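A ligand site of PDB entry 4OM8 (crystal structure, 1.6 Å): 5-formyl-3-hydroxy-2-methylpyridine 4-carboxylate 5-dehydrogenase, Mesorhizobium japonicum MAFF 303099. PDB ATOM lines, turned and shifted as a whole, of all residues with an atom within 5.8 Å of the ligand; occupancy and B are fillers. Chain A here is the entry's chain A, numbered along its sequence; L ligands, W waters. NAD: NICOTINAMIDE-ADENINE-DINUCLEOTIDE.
OD2 of Asp 32 lies within hydrogen-bond range of O3B of the ligand (2.6 Å). The side-chain carboxylate of Glu 89 sits at hydrogen-bond distance from an oxygen (O3D) of the ligand, 2.8 Å away. N of Thr 12 sits at hydrogen-bond distance from O2A of the ligand (3.0 Å). The side-chain hydroxyl (OG1) of Thr 12 is in hydrogen-bond range of an oxygen (O2A) of the ligand (3.2 Å). The backbone NH of Met 13 sits at hydrogen-bond distance from an oxygen (O2N) of the ligand (3.0 Å). An oxygen (O3D) of the ligand sits at hydrogen-bond distance from the side-chain amino group of Lys 94. The side-chain amide oxygen (OD1) of Asn 86 sits close to an oxygen (O4D) of the ligand (3.2 Å). O of Val 87 sits close to O3D of the ligand, at 3.3 Å.
Water W2 lies within hydrogen-bond range of an oxygen (O1N) of the ligand (2.4 Å) and the side-chain hydroxyl (OG1) of Thr 12 (2.9 Å). Water W9 bridges an oxygen (O3B) of the ligand (2.7 Å) and the guanidinium group of Arg 40 (3.2 Å). Water W11 lies within hydrogen-bond range of the backbone NH (N) of Gly 11, an oxygen (O2N) of the ligand and the backbone carbonyl oxygen (O) of Asn 86. Water W7 lies within hydrogen-bond range of the backbone NH of Asn 140 (2.8 Å) and a nitrogen (N7N) of the ligand (3.5 Å).
O4D of the ligand lies close to OD2 of Asp 114 (3.2 Å). Residues that only touch the ligand: Trp 138 (3.1 Å), Pro 88 (3.3 Å), Gly 11 (3.3 Å), Ser 116 (3.4 Å), Ile 8 (3.5 Å), Asn 140 (3.5 Å), Val 33 (3.5 Å), Ala 37 (3.6 Å), Thr 115 (3.6 Å), Tyr 31 (3.6 Å), His 137 (3.7 Å), Val 97 (3.7 Å), Ala 34 (3.7 Å), Ile 93 (3.8 Å), Gly 9 (3.9 Å) and Leu 10 (3.999 Å). Hydrophobic or aromatic side chains within 4 Å of the ligand: Ile 8, Met 13, Tyr 31, Val 33, Ala 34, Ala 37, Val 87, Pro 88, Ile 93, Val 97 and His 137. Within 4 Å of the ligand: Ile 8, Gly 9, Leu 10, Gly 11, Thr 12, Met 13, Tyr 31, Asp 32, Val 33, Ala 34, Ala 37, Asn 86, Val 87, Pro 88, Glu 89, Ile 93, Lys 94, Val 97, Asp 114, Thr 115, Ser 116, His 137, Trp 138 and Asn 140.
The side-chain carboxylate of Asp 32 is in hydrogen-bond range of the backbone NH of Ala 34 (2.9 Å). The backbone NH (N) of Leu 10 is in hydrogen-bond range of the side-chain carboxylate (OD2) of Asp 32 (2.8 Å). The side-chain carboxylate of Glu 89 is in hydrogen-bond range of the backbone NH of Ser 116 (3.2 Å). OE1 of Glu 89 is in hydrogen-bond range of N of Gly 117 (2.6 Å). The side-chain amide oxygen of Asn 86 sits close to the side-chain carboxylate of Asp 114, 2.7 Å away. The backbone NH of Asp 114 lies within hydrogen-bond range of the backbone carbonyl oxygen of Glu 85. N of Asn 86 sits at hydrogen-bond distance from O of Ile 8, 2.7 Å away. The side-chain amide nitrogen (ND2) of Asn 86 sits at hydrogen-bond distance from the backbone carbonyl oxygen (O) of Gly 9 (3.0 Å).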
ATOM      1  N   ILE A   8      14.828 -28.904   1.034  1.00  0.00           N
ATOM      2  CA  ILE A   8      14.393 -29.921   0.080  1.00  0.00           C
ATOM      3  C   ILE A   8      13.750 -29.245  -1.125  1.00  0.00           C
ATOM      4  O   ILE A   8      12.638 -28.717  -1.031  1.00  0.00           O
ATOM      5  CB  ILE A   8      13.386 -30.896   0.711  1.00  0.00           C
ATOM      6  CG1 ILE A   8      13.929 -31.414   2.048  1.00  0.00           C
ATOM      7  CG2 ILE A   8      13.019 -32.015  -0.272  1.00  0.00           C
ATOM      8  CD1 ILE A   8      15.296 -32.092   1.979  1.00  0.00           C
ATOM      9  N   GLY A   9      14.483 -29.215  -2.234  1.00  0.00           N
ATOM     10  CA  GLY A   9      13.996 -28.589  -3.459  1.00  0.00           C
ATOM     11  C   GLY A   9      14.846 -27.389  -3.770  1.00  0.00           C
ATOM     12  O   GLY A   9      14.914 -26.440  -2.980  1.00  0.00           O
ATOM     13  N   LEU A  10      15.509 -27.429  -4.932  1.00  0.00           N
ATOM     14  CA  LEU A  10      16.477 -26.411  -5.333  1.00  0.00           C
ATOM     15  C   LEU A  10      16.174 -25.760  -6.670  1.00  0.00           C
ATOM     16  O   LEU A  10      17.087 -25.557  -7.484  1.00  0.00           O
ATOM     17  CB  LEU A  10      17.880 -27.009  -5.396  1.00  0.00           C
ATOM     18  CG  LEU A  10      18.607 -27.297  -4.088  1.00  0.00           C
ATOM     19  CD1 LEU A  10      19.898 -28.054  -4.375  1.00  0.00           C
ATOM     20  CD2 LEU A  10      18.898 -25.990  -3.377  1.00  0.00           C
ATOM     21  N   GLY A  11      14.917 -25.443  -6.915  1.00  0.00           N
ATOM     22  CA  GLY A  11      14.542 -24.744  -8.136  1.00  0.00           C
ATOM     23  C   GLY A  11      14.745 -23.262  -7.952  1.00  0.00           C
ATOM     24  O   GLY A  11      15.719 -22.826  -7.351  1.00  0.00           O
ATOM     25  N   THR A  12      13.810 -22.471  -8.472  1.00  0.00           N
ATOM     26  CA  THR A  12      13.845 -21.023  -8.398  1.00  0.00           C
ATOM     27  C   THR A  12      14.167 -20.476  -7.011  1.00  0.00           C
ATOM     28  O   THR A  12      14.990 -19.571  -6.873  1.00  0.00           O
ATOM     29  CB  THR A  12      12.502 -20.456  -8.878  1.00  0.00           C
ATOM     30  OG1 THR A  12      12.286 -20.855 -10.230  1.00  0.00           O
ATOM     31  CG2 THR A  12      12.468 -18.935  -8.765  1.00  0.00           C
ATOM     32  N   MET A  13      13.521 -21.046  -5.992  1.00  0.00           N
ATOM     33  CA  MET A  13      13.612 -20.474  -4.639  1.00  0.00           C
ATOM     34  C   MET A  13      14.759 -21.035  -3.793  1.00  0.00           C
ATOM     35  O   MET A  13      15.034 -20.528  -2.709  1.00  0.00           O
ATOM     36  CB  MET A  13      12.301 -20.689  -3.886  1.00  0.00           C
ATOM     37  CG  MET A  13      11.134 -19.932  -4.464  1.00  0.00           C
ATOM     38  SD  MET A  13      11.392 -18.156  -4.374  1.00  0.00           S
ATOM     39  CE  MET A  13      11.119 -17.855  -2.637  1.00  0.00           C
ATOM     40  N   GLY A  14      15.412 -22.079  -4.285  1.00  0.00           N
ATOM     41  CA  GLY A  14      16.355 -22.814  -3.449  1.00  0.00           C
ATOM     42  C   GLY A  14      17.731 -22.214  -3.194  1.00  0.00           C
ATOM     43  O   GLY A  14      18.136 -22.041  -2.036  1.00  0.00           O
ATOM     44  N   TYR A  31      19.062 -30.482  -0.931  1.00  0.00           N
ATOM     45  CA  TYR A  31      18.818 -31.682  -1.714  1.00  0.00           C
ATOM     46  C   TYR A  31      17.803 -31.426  -2.800  1.00  0.00           C
ATOM     47  O   TYR A  31      16.880 -30.658  -2.602  1.00  0.00           O
ATOM     48  CB  TYR A  31      18.332 -32.816  -0.804  1.00  0.00           C
ATOM     49  CG  TYR A  31      17.709 -34.000  -1.518  1.00  0.00           C
ATOM     50  CD1 TYR A  31      18.500 -35.011  -2.047  1.00  0.00           C
ATOM     51  CD2 TYR A  31      16.336 -34.103  -1.668  1.00  0.00           C
ATOM     52  CE1 TYR A  31      17.940 -36.103  -2.710  1.00  0.00           C
ATOM     53  CE2 TYR A  31      15.761 -35.184  -2.314  1.00  0.00           C
ATOM     54  CZ  TYR A  31      16.563 -36.168  -2.844  1.00  0.00           C
ATOM     55  OH  TYR A  31      15.972 -37.231  -3.492  1.00  0.00           O
ATOM     56  N   ASP A  32      17.966 -32.089  -3.930  1.00  0.00           N
ATOM     57  CA  ASP A  32      16.939 -32.067  -4.968  1.00  0.00           C
ATOM     58  C   ASP A  32      16.939 -33.449  -5.618  1.00  0.00           C
ATOM     59  O   ASP A  32      17.987 -34.063  -5.749  1.00  0.00           O
ATOM     60  CB  ASP A  32      17.218 -30.973  -6.007  1.00  0.00           C
ATOM     61  CG  ASP A  32      15.987 -30.651  -6.874  1.00  0.00           C
ATOM     62  OD1 ASP A  32      15.535 -31.538  -7.621  1.00  0.00           O
ATOM     63  OD2 ASP A  32      15.509 -29.490  -6.805  1.00  0.00           O
ATOM     64  N   VAL A  33      15.757 -33.904  -6.036  1.00  0.00           N
ATOM     65  CA  VAL A  33      15.590 -35.206  -6.663  1.00  0.00           C
ATOM     66  C   VAL A  33      16.191 -35.242  -8.086  1.00  0.00           C
ATOM     67  O   VAL A  33      16.465 -36.323  -8.618  1.00  0.00           O
ATOM     68  CB  VAL A  33      14.095 -35.597  -6.708  1.00  0.00           C
ATOM     69  CG1 VAL A  33      13.365 -34.771  -7.753  1.00  0.00           C
ATOM     70  CG2 VAL A  33      13.911 -37.100  -6.958  1.00  0.00           C
ATOM     71  N   ALA A  34      16.386 -34.074  -8.693  1.00  0.00           N
ATOM     72  CA  ALA A  34      16.820 -34.001 -10.082  1.00  0.00           C
ATOM     73  C   ALA A  34      18.250 -33.513 -10.196  1.00  0.00           C
ATOM     74  O   ALA A  34      18.547 -32.390  -9.811  1.00  0.00           O
ATOM     75  CB  ALA A  34      15.895 -33.081 -10.877  1.00  0.00           C
ATOM     76  N   ALA A  37      18.800 -30.157 -11.667  1.00  0.00           N
ATOM     77  CA  ALA A  37      18.465 -29.064 -10.752  1.00  0.00           C
ATOM     78  C   ALA A  37      19.616 -28.716  -9.819  1.00  0.00           C
ATOM     79  O   ALA A  37      19.873 -27.541  -9.528  1.00  0.00           O
ATOM     80  CB  ALA A  37      17.236 -29.423  -9.949  1.00  0.00           C
ATOM     81  N   ARG A  40      22.227 -26.781 -11.843  1.00  0.00           N
ATOM     82  CA  ARG A  40      21.774 -25.413 -12.106  1.00  0.00           C
ATOM     83  C   ARG A  40      21.897 -24.572 -10.833  1.00  0.00           C
ATOM     84  O   ARG A  40      22.252 -23.393 -10.880  1.00  0.00           O
ATOM     85  CB  ARG A  40      20.330 -25.398 -12.623  1.00  0.00           C
ATOM     86  CG  ARG A  40      20.169 -25.859 -14.073  1.00  0.00           C
ATOM     87  CD  ARG A  40      18.773 -25.529 -14.632  1.00  0.00           C
ATOM     88  NE  ARG A  40      17.711 -26.263 -13.939  1.00  0.00           N
ATOM     89  CZ  ARG A  40      17.284 -27.469 -14.296  1.00  0.00           C
ATOM     90  NH1 ARG A  40      17.814 -28.091 -15.328  1.00  0.00           N
ATOM     91  NH2 ARG A  40      16.308 -28.054 -13.608  1.00  0.00           N
ATOM     92  N   ILE A  73      18.888 -37.747   0.377  1.00  0.00           N
ATOM     93  CA  ILE A  73      18.047 -36.962   1.289  1.00  0.00           C
ATOM     94  C   ILE A  73      18.343 -37.298   2.766  1.00  0.00           C
ATOM     95  O   ILE A  73      18.215 -36.429   3.627  1.00  0.00           O
ATOM     96  CB  ILE A  73      16.557 -37.152   0.956  1.00  0.00           C
ATOM     97  CG1 ILE A  73      15.715 -36.058   1.646  1.00  0.00           C
ATOM     98  CG2 ILE A  73      16.088 -38.557   1.307  1.00  0.00           C
ATOM     99  CD1 ILE A  73      14.285 -35.994   1.136  1.00  0.00           C
ATOM    100  N   GLU A  85      10.837 -27.453   3.394  1.00  0.00           N
ATOM    101  CA  GLU A  85      10.337 -28.132   2.206  1.00  0.00           C
ATOM    102  C   GLU A  85      10.019 -27.089   1.139  1.00  0.00           C
ATOM    103  O   GLU A  85       9.275 -26.111   1.398  1.00  0.00           O
ATOM    104  CB  GLU A  85       9.111 -28.990   2.533  1.00  0.00           C
ATOM    105  CG  GLU A  85       8.382 -29.502   1.302  1.00  0.00           C
ATOM    106  CD  GLU A  85       7.344 -28.512   0.823  1.00  0.00           C
ATOM    107  OE1 GLU A  85       6.450 -28.171   1.626  1.00  0.00           O
ATOM    108  OE2 GLU A  85       7.408 -28.092  -0.353  1.00  0.00           O
ATOM    109  N   ASN A  86      10.582 -27.295  -0.044  1.00  0.00           N
ATOM    110  CA  ASN A  86      10.566 -26.297  -1.104  1.00  0.00           C
ATOM    111  C   ASN A  86      10.390 -26.986  -2.471  1.00  0.00           C
ATOM    112  O   ASN A  86      11.097 -26.680  -3.421  1.00  0.00           O
ATOM    113  CB  ASN A  86      11.871 -25.492  -1.050  1.00  0.00           C
ATOM    114  CG  ASN A  86      11.887 -24.288  -1.977  1.00  0.00           C
ATOM    115  OD1 ASN A  86      10.930 -23.510  -2.031  1.00  0.00           O
ATOM    116  ND2 ASN A  86      12.977 -24.141  -2.706  1.00  0.00           N
ATOM    117  N   VAL A  87       9.453 -27.932  -2.534  1.00  0.00           N
ATOM    118  CA  VAL A  87       9.246 -28.746  -3.730  1.00  0.00           C
ATOM    119  C   VAL A  87       8.015 -28.189  -4.479  1.00  0.00           C
ATOM    120  O   VAL A  87       7.445 -27.199  -4.032  1.00  0.00           O
ATOM    121  CB  VAL A  87       9.100 -30.253  -3.356  1.00  0.00           C
ATOM    122  CG1 VAL A  87      10.346 -30.732  -2.587  1.00  0.00           C
ATOM    123  CG2 VAL A  87       7.791 -30.534  -2.608  1.00  0.00           C
ATOM    124  N   PRO A  88       7.629 -28.773  -5.634  1.00  0.00           N
ATOM    125  CA  PRO A  88       6.527 -28.160  -6.378  1.00  0.00           C
ATOM    126  C   PRO A  88       5.231 -28.002  -5.594  1.00  0.00           C
ATOM    127  O   PRO A  88       4.975 -28.682  -4.585  1.00  0.00           O
ATOM    128  CB  PRO A  88       6.310 -29.128  -7.548  1.00  0.00           C
ATOM    129  CG  PRO A  88       7.657 -29.714  -7.784  1.00  0.00           C
ATOM    130  CD  PRO A  88       8.299 -29.825  -6.425  1.00  0.00           C
ATOM    131  N   GLU A  89       4.418 -27.076  -6.087  1.00  0.00           N
ATOM    132  CA  GLU A  89       3.137 -26.748  -5.486  1.00  0.00           C
ATOM    133  C   GLU A  89       2.084 -27.835  -5.787  1.00  0.00           C
ATOM    134  O   GLU A  89       1.200 -27.655  -6.628  1.00  0.00           O
ATOM    135  CB  GLU A  89       2.696 -25.376  -5.978  1.00  0.00           C
ATOM    136  CG  GLU A  89       1.549 -24.799  -5.207  1.00  0.00           C
ATOM    137  CD  GLU A  89       1.978 -24.194  -3.887  1.00  0.00           C
ATOM    138  OE1 GLU A  89       1.382 -23.157  -3.536  1.00  0.00           O
ATOM    139  OE2 GLU A  89       2.877 -24.740  -3.197  1.00  0.00           O
ATOM    140  N   ILE A  93       3.072 -34.419  -3.836  1.00  0.00           N
ATOM    141  CA  ILE A  93       4.538 -34.390  -3.804  1.00  0.00           C
ATOM    142  C   ILE A  93       5.045 -33.916  -2.439  1.00  0.00           C
ATOM    143  O   ILE A  93       5.988 -34.493  -1.898  1.00  0.00           O
ATOM    144  CB  ILE A  93       5.122 -33.496  -4.923  1.00  0.00           C
ATOM    145  CG1 ILE A  93       4.674 -34.016  -6.293  1.00  0.00           C
ATOM    146  CG2 ILE A  93       6.639 -33.465  -4.854  1.00  0.00           C
ATOM    147  CD1 ILE A  93       5.264 -33.256  -7.467  1.00  0.00           C
ATOM    148  N   LYS A  94       4.418 -32.886  -1.870  1.00  0.00           N
ATOM    149  CA  LYS A  94       4.848 -32.404  -0.556  1.00  0.00           C
ATOM    150  C   LYS A  94       4.630 -33.491   0.511  1.00  0.00           C
ATOM    151  O   LYS A  94       5.498 -33.714   1.358  1.00  0.00           O
ATOM    152  CB  LYS A  94       4.110 -31.118  -0.183  1.00  0.00           C
ATOM    153  CG  LYS A  94       4.393 -29.949  -1.127  1.00  0.00           C
ATOM    154  CD  LYS A  94       3.864 -28.629  -0.583  1.00  0.00           C
ATOM    155  CE  LYS A  94       4.018 -27.511  -1.596  1.00  0.00           C
ATOM    156  NZ  LYS A  94       5.426 -27.339  -2.075  1.00  0.00           N
ATOM    157  N   ASP A  96       4.678 -36.681   0.010  1.00  0.00           N
ATOM    158  CA  ASP A  96       5.742 -37.662  -0.218  1.00  0.00           C
ATOM    159  C   ASP A  96       7.015 -37.263   0.524  1.00  0.00           C
ATOM    160  O   ASP A  96       7.666 -38.095   1.163  1.00  0.00           O
ATOM    161  CB  ASP A  96       6.058 -37.794  -1.707  1.00  0.00           C
ATOM    162  CG  ASP A  96       4.971 -38.504  -2.481  1.00  0.00           C
ATOM    163  OD1 ASP A  96       4.182 -39.256  -1.864  1.00  0.00           O
ATOM    164  OD2 ASP A  96       4.908 -38.323  -3.715  1.00  0.00           O
ATOM    165  N   VAL A  97       7.366 -35.984   0.431  1.00  0.00           N
ATOM    166  CA  VAL A  97       8.563 -35.488   1.103  1.00  0.00           C
ATOM    167  C   VAL A  97       8.413 -35.646   2.626  1.00  0.00           C
ATOM    168  O   VAL A  97       9.326 -36.141   3.291  1.00  0.00           O
ATOM    169  CB  VAL A  97       8.838 -34.014   0.752  1.00  0.00           C
ATOM    170  CG1 VAL A  97       9.910 -33.443   1.667  1.00  0.00           C
ATOM    171  CG2 VAL A  97       9.264 -33.887  -0.712  1.00  0.00           C
ATOM    172  N   SER A 113       7.145 -25.250   5.334  1.00  0.00           N
ATOM    173  CA  SER A 113       6.890 -25.268   3.903  1.00  0.00           C
ATOM    174  C   SER A 113       6.984 -23.878   3.314  1.00  0.00           C
ATOM    175  O   SER A 113       6.488 -22.919   3.913  1.00  0.00           O
ATOM    176  CB  SER A 113       5.503 -25.838   3.597  1.00  0.00           C
ATOM    177  OG  SER A 113       5.268 -25.823   2.187  1.00  0.00           O
ATOM    178  N   ASP A 114       7.590 -23.788   2.126  1.00  0.00           N
ATOM    179  CA  ASP A 114       7.645 -22.548   1.351  1.00  0.00           C
ATOM    180  C   ASP A 114       6.388 -22.364   0.485  1.00  0.00           C
ATOM    181  O   ASP A 114       6.342 -21.436  -0.317  1.00  0.00           O
ATOM    182  CB  ASP A 114       8.900 -22.560   0.469  1.00  0.00           C
ATOM    183  CG  ASP A 114       9.279 -21.195  -0.093  1.00  0.00           C
ATOM    184  OD1 ASP A 114       8.960 -20.168   0.521  1.00  0.00           O
ATOM    185  OD2 ASP A 114       9.969 -21.166  -1.132  1.00  0.00           O
ATOM    186  N   THR A 115       5.386 -23.222   0.663  1.00  0.00           N
ATOM    187  CA  THR A 115       4.174 -23.163  -0.172  1.00  0.00           C
ATOM    188  C   THR A 115       3.562 -21.773  -0.231  1.00  0.00           C
ATOM    189  O   THR A 115       3.544 -21.034   0.747  1.00  0.00           O
ATOM    190  CB  THR A 115       3.099 -24.153   0.310  1.00  0.00           C
ATOM    191  OG1 THR A 115       2.000 -24.140  -0.614  1.00  0.00           O
ATOM    192  CG2 THR A 115       2.587 -23.769   1.700  1.00  0.00           C
ATOM    193  N   SER A 116       3.052 -21.409  -1.407  1.00  0.00           N
ATOM    194  CA  SER A 116       2.286 -20.178  -1.542  1.00  0.00           C
ATOM    195  C   SER A 116       0.789 -20.394  -1.340  1.00  0.00           C
ATOM    196  O   SER A 116       0.107 -19.537  -0.790  1.00  0.00           O
ATOM    197  CB  SER A 116       2.547 -19.562  -2.915  1.00  0.00           C
ATOM    198  OG  SER A 116       3.900 -19.155  -3.040  1.00  0.00           O
ATOM    199  N   GLY A 117       0.265 -21.531  -1.798  1.00  0.00           N
ATOM    200  CA  GLY A 117      -1.172 -21.668  -1.899  1.00  0.00           C
ATOM    201  C   GLY A 117      -1.831 -22.876  -1.268  1.00  0.00           C
ATOM    202  O   GLY A 117      -3.053 -23.020  -1.336  1.00  0.00           O
ATOM    203  N   HIS A 137       7.105 -18.643   4.309  1.00  0.00           N
ATOM    204  CA  HIS A 137       6.870 -18.304   2.923  1.00  0.00           C
ATOM    205  C   HIS A 137       7.774 -17.163   2.482  1.00  0.00           C
ATOM    206  O   HIS A 137       7.575 -16.018   2.856  1.00  0.00           O
ATOM    207  CB  HIS A 137       5.400 -17.955   2.719  1.00  0.00           C
ATOM    208  CG  HIS A 137       5.072 -17.560   1.314  1.00  0.00           C
ATOM    209  ND1 HIS A 137       4.645 -16.295   0.995  1.00  0.00           N
ATOM    210  CD2 HIS A 137       5.109 -18.260   0.164  1.00  0.00           C
ATOM    211  CE1 HIS A 137       4.424 -16.232  -0.310  1.00  0.00           C
ATOM    212  NE2 HIS A 137       4.690 -17.411  -0.837  1.00  0.00           N
ATOM    213  N   TRP A 138       8.801 -17.521   1.719  1.00  0.00           N
ATOM    214  CA  TRP A 138       9.752 -16.570   1.173  1.00  0.00           C
ATOM    215  C   TRP A 138       9.200 -15.937  -0.095  1.00  0.00           C
ATOM    216  O   TRP A 138       8.165 -16.355  -0.604  1.00  0.00           O
ATOM    217  CB  TRP A 138      11.067 -17.272   0.861  1.00  0.00           C
ATOM    218  CG  TRP A 138      11.774 -17.889   2.038  1.00  0.00           C
ATOM    219  CD1 TRP A 138      11.331 -18.904   2.848  1.00  0.00           C
ATOM    220  CD2 TRP A 138      13.078 -17.539   2.505  1.00  0.00           C
ATOM    221  NE1 TRP A 138      12.287 -19.200   3.796  1.00  0.00           N
ATOM    222  CE2 TRP A 138      13.366 -18.380   3.614  1.00  0.00           C
ATOM    223  CE3 TRP A 138      14.033 -16.602   2.094  1.00  0.00           C
ATOM    224  CZ2 TRP A 138      14.572 -18.298   4.312  1.00  0.00           C
ATOM    225  CZ3 TRP A 138      15.227 -16.518   2.805  1.00  0.00           C
ATOM    226  CH2 TRP A 138      15.488 -17.370   3.891  1.00  0.00           C
ATOM    227  N   SER A 139       9.905 -14.923  -0.593  1.00  0.00           N
ATOM    228  CA  SER A 139       9.529 -14.278  -1.847  1.00  0.00           C
ATOM    229  C   SER A 139      10.675 -14.309  -2.852  1.00  0.00           C
ATOM    230  O   SER A 139      11.846 -14.357  -2.453  1.00  0.00           O
ATOM    231  CB  SER A 139       9.075 -12.832  -1.599  1.00  0.00           C
ATOM    232  OG  SER A 139       7.850 -12.781  -0.879  1.00  0.00           O
ATOM    233  N   ASN A 140      10.362 -14.286  -4.139  1.00  0.00           N
ATOM    234  CA  ASN A 140      11.385 -14.357  -5.177  1.00  0.00           C
ATOM    235  C   ASN A 140      11.905 -12.977  -5.533  1.00  0.00           C
ATOM    236  O   ASN A 140      11.105 -12.095  -5.817  1.00  0.00           O
ATOM    237  CB  ASN A 140      10.803 -15.045  -6.412  1.00  0.00           C
ATOM    238  CG  ASN A 140      11.846 -15.260  -7.500  1.00  0.00           C
ATOM    239  OD1 ASN A 140      12.993 -15.595  -7.226  1.00  0.00           O
ATOM    240  ND2 ASN A 140      11.416 -15.090  -8.744  1.00  0.00           N
HETATM  241  PA  NAD L   1      10.530 -24.963  -8.902  1.00  0.00           P
HETATM  242  O1A NAD L   1       9.593 -25.765  -9.788  1.00  0.00           O
HETATM  243  O2A NAD L   1      11.431 -23.900  -9.505  1.00  0.00           O
HETATM  244  O5B NAD L   1      11.458 -26.010  -8.105  1.00  0.00           O
HETATM  245  C5B NAD L   1      10.942 -27.203  -7.520  1.00  0.00           C
HETATM  246  C4B NAD L   1      12.107 -28.153  -7.281  1.00  0.00           C
HETATM  247  O4B NAD L   1      11.662 -29.251  -6.493  1.00  0.00           O
HETATM  248  C3B NAD L   1      12.639 -28.715  -8.594  1.00  0.00           C
HETATM  249  O3B NAD L   1      14.043 -28.452  -8.720  1.00  0.00           O
HETATM  250  C2B NAD L   1      12.340 -30.204  -8.507  1.00  0.00           C
HETATM  251  O2B NAD L   1      13.304 -31.043  -9.153  1.00  0.00           O
HETATM  252  C1B NAD L   1      12.337 -30.417  -7.004  1.00  0.00           C
HETATM  253  N9A NAD L   1      11.636 -31.620  -6.518  1.00  0.00           N
HETATM  254  C8A NAD L   1      10.529 -32.193  -7.027  1.00  0.00           C
HETATM  255  N7A NAD L   1      10.173 -33.272  -6.286  1.00  0.00           N
HETATM  256  C5A NAD L   1      11.054 -33.390  -5.278  1.00  0.00           C
HETATM  257  C6A NAD L   1      11.273 -34.303  -4.145  1.00  0.00           C
HETATM  258  N6A NAD L   1      10.432 -35.348  -3.913  1.00  0.00           N
HETATM  259  N1A NAD L   1      12.327 -34.068  -3.343  1.00  0.00           N
HETATM  260  C2A NAD L   1      13.176 -33.048  -3.565  1.00  0.00           C
HETATM  261  N3A NAD L   1      13.035 -32.176  -4.572  1.00  0.00           N
HETATM  262  C4A NAD L   1      12.017 -32.303  -5.455  1.00  0.00           C
HETATM  263  O3  NAD L   1       9.635 -24.393  -7.690  1.00  0.00           O
HETATM  264  PN  NAD L   1       9.861 -23.022  -6.890  1.00  0.00           P
HETATM  265  O1N NAD L   1       9.369 -21.856  -7.730  1.00  0.00           O
HETATM  266  O2N NAD L   1      11.238 -22.941  -6.281  1.00  0.00           O
HETATM  267  O5D NAD L   1       8.807 -23.198  -5.688  1.00  0.00           O
HETATM  268  C5D NAD L   1       8.956 -24.211  -4.694  1.00  0.00           C
HETATM  269  C4D NAD L   1       7.888 -23.983  -3.630  1.00  0.00           C
HETATM  270  O4D NAD L   1       8.035 -22.651  -3.162  1.00  0.00           O
HETATM  271  C3D NAD L   1       6.477 -24.091  -4.180  1.00  0.00           C
HETATM  272  O3D NAD L   1       5.640 -24.541  -3.119  1.00  0.00           O
HETATM  273  C2D NAD L   1       6.108 -22.659  -4.516  1.00  0.00           C
HETATM  274  O2D NAD L   1       4.698 -22.427  -4.416  1.00  0.00           O
HETATM  275  C1D NAD L   1       6.844 -21.893  -3.432  1.00  0.00           C
HETATM  276  N1N NAD L   1       7.203 -20.508  -3.776  1.00  0.00           N
HETATM  277  C2N NAD L   1       7.504 -20.127  -5.033  1.00  0.00           C
HETATM  278  C3N NAD L   1       7.854 -18.806  -5.293  1.00  0.00           C
HETATM  279  C7N NAD L   1       8.166 -18.301  -6.686  1.00  0.00           C
HETATM  280  O7N NAD L   1       8.609 -19.043  -7.548  1.00  0.00           O
HETATM  281  N7N NAD L   1       7.913 -17.018  -6.934  1.00  0.00           N
HETATM  282  C4N NAD L   1       7.897 -17.885  -4.260  1.00  0.00           C
HETATM  283  C5N NAD L   1       7.590 -18.309  -2.965  1.00  0.00           C
HETATM  284  C6N NAD L   1       7.254 -19.637  -2.754  1.00  0.00           C
HETATM  285  O   HOH W   1       8.525 -18.640 -10.376  1.00  0.00           O
HETATM  286  O   HOH W   2       9.437 -21.265 -10.089  1.00  0.00           O
HETATM  287  O   HOH W   3       9.009 -23.372 -12.173  1.00  0.00           O
HETATM  288  O   HOH W   4       9.506 -31.407 -10.268  1.00  0.00           O
HETATM  289  O   HOH W   5      10.209 -27.861 -11.552  1.00  0.00           O
HETATM  290  O   HOH W   6       4.464 -18.574  -5.796  1.00  0.00           O
HETATM  291  O   HOH W   7       7.696 -14.169  -4.983  1.00  0.00           O
HETATM  292  O   HOH W   8       6.486 -22.104  -7.921  1.00  0.00           O
HETATM  293  O   HOH W   9      14.363 -27.343 -11.151  1.00  0.00           O
HETATM  294  O   HOH W  10       6.739 -25.700 -10.160  1.00  0.00           O
HETATM  295  O   HOH W  11      12.613 -25.219  -5.349  1.00  0.00           O
HETATM  296  O   HOH W  12      11.939 -32.860 -10.688  1.00  0.00           O
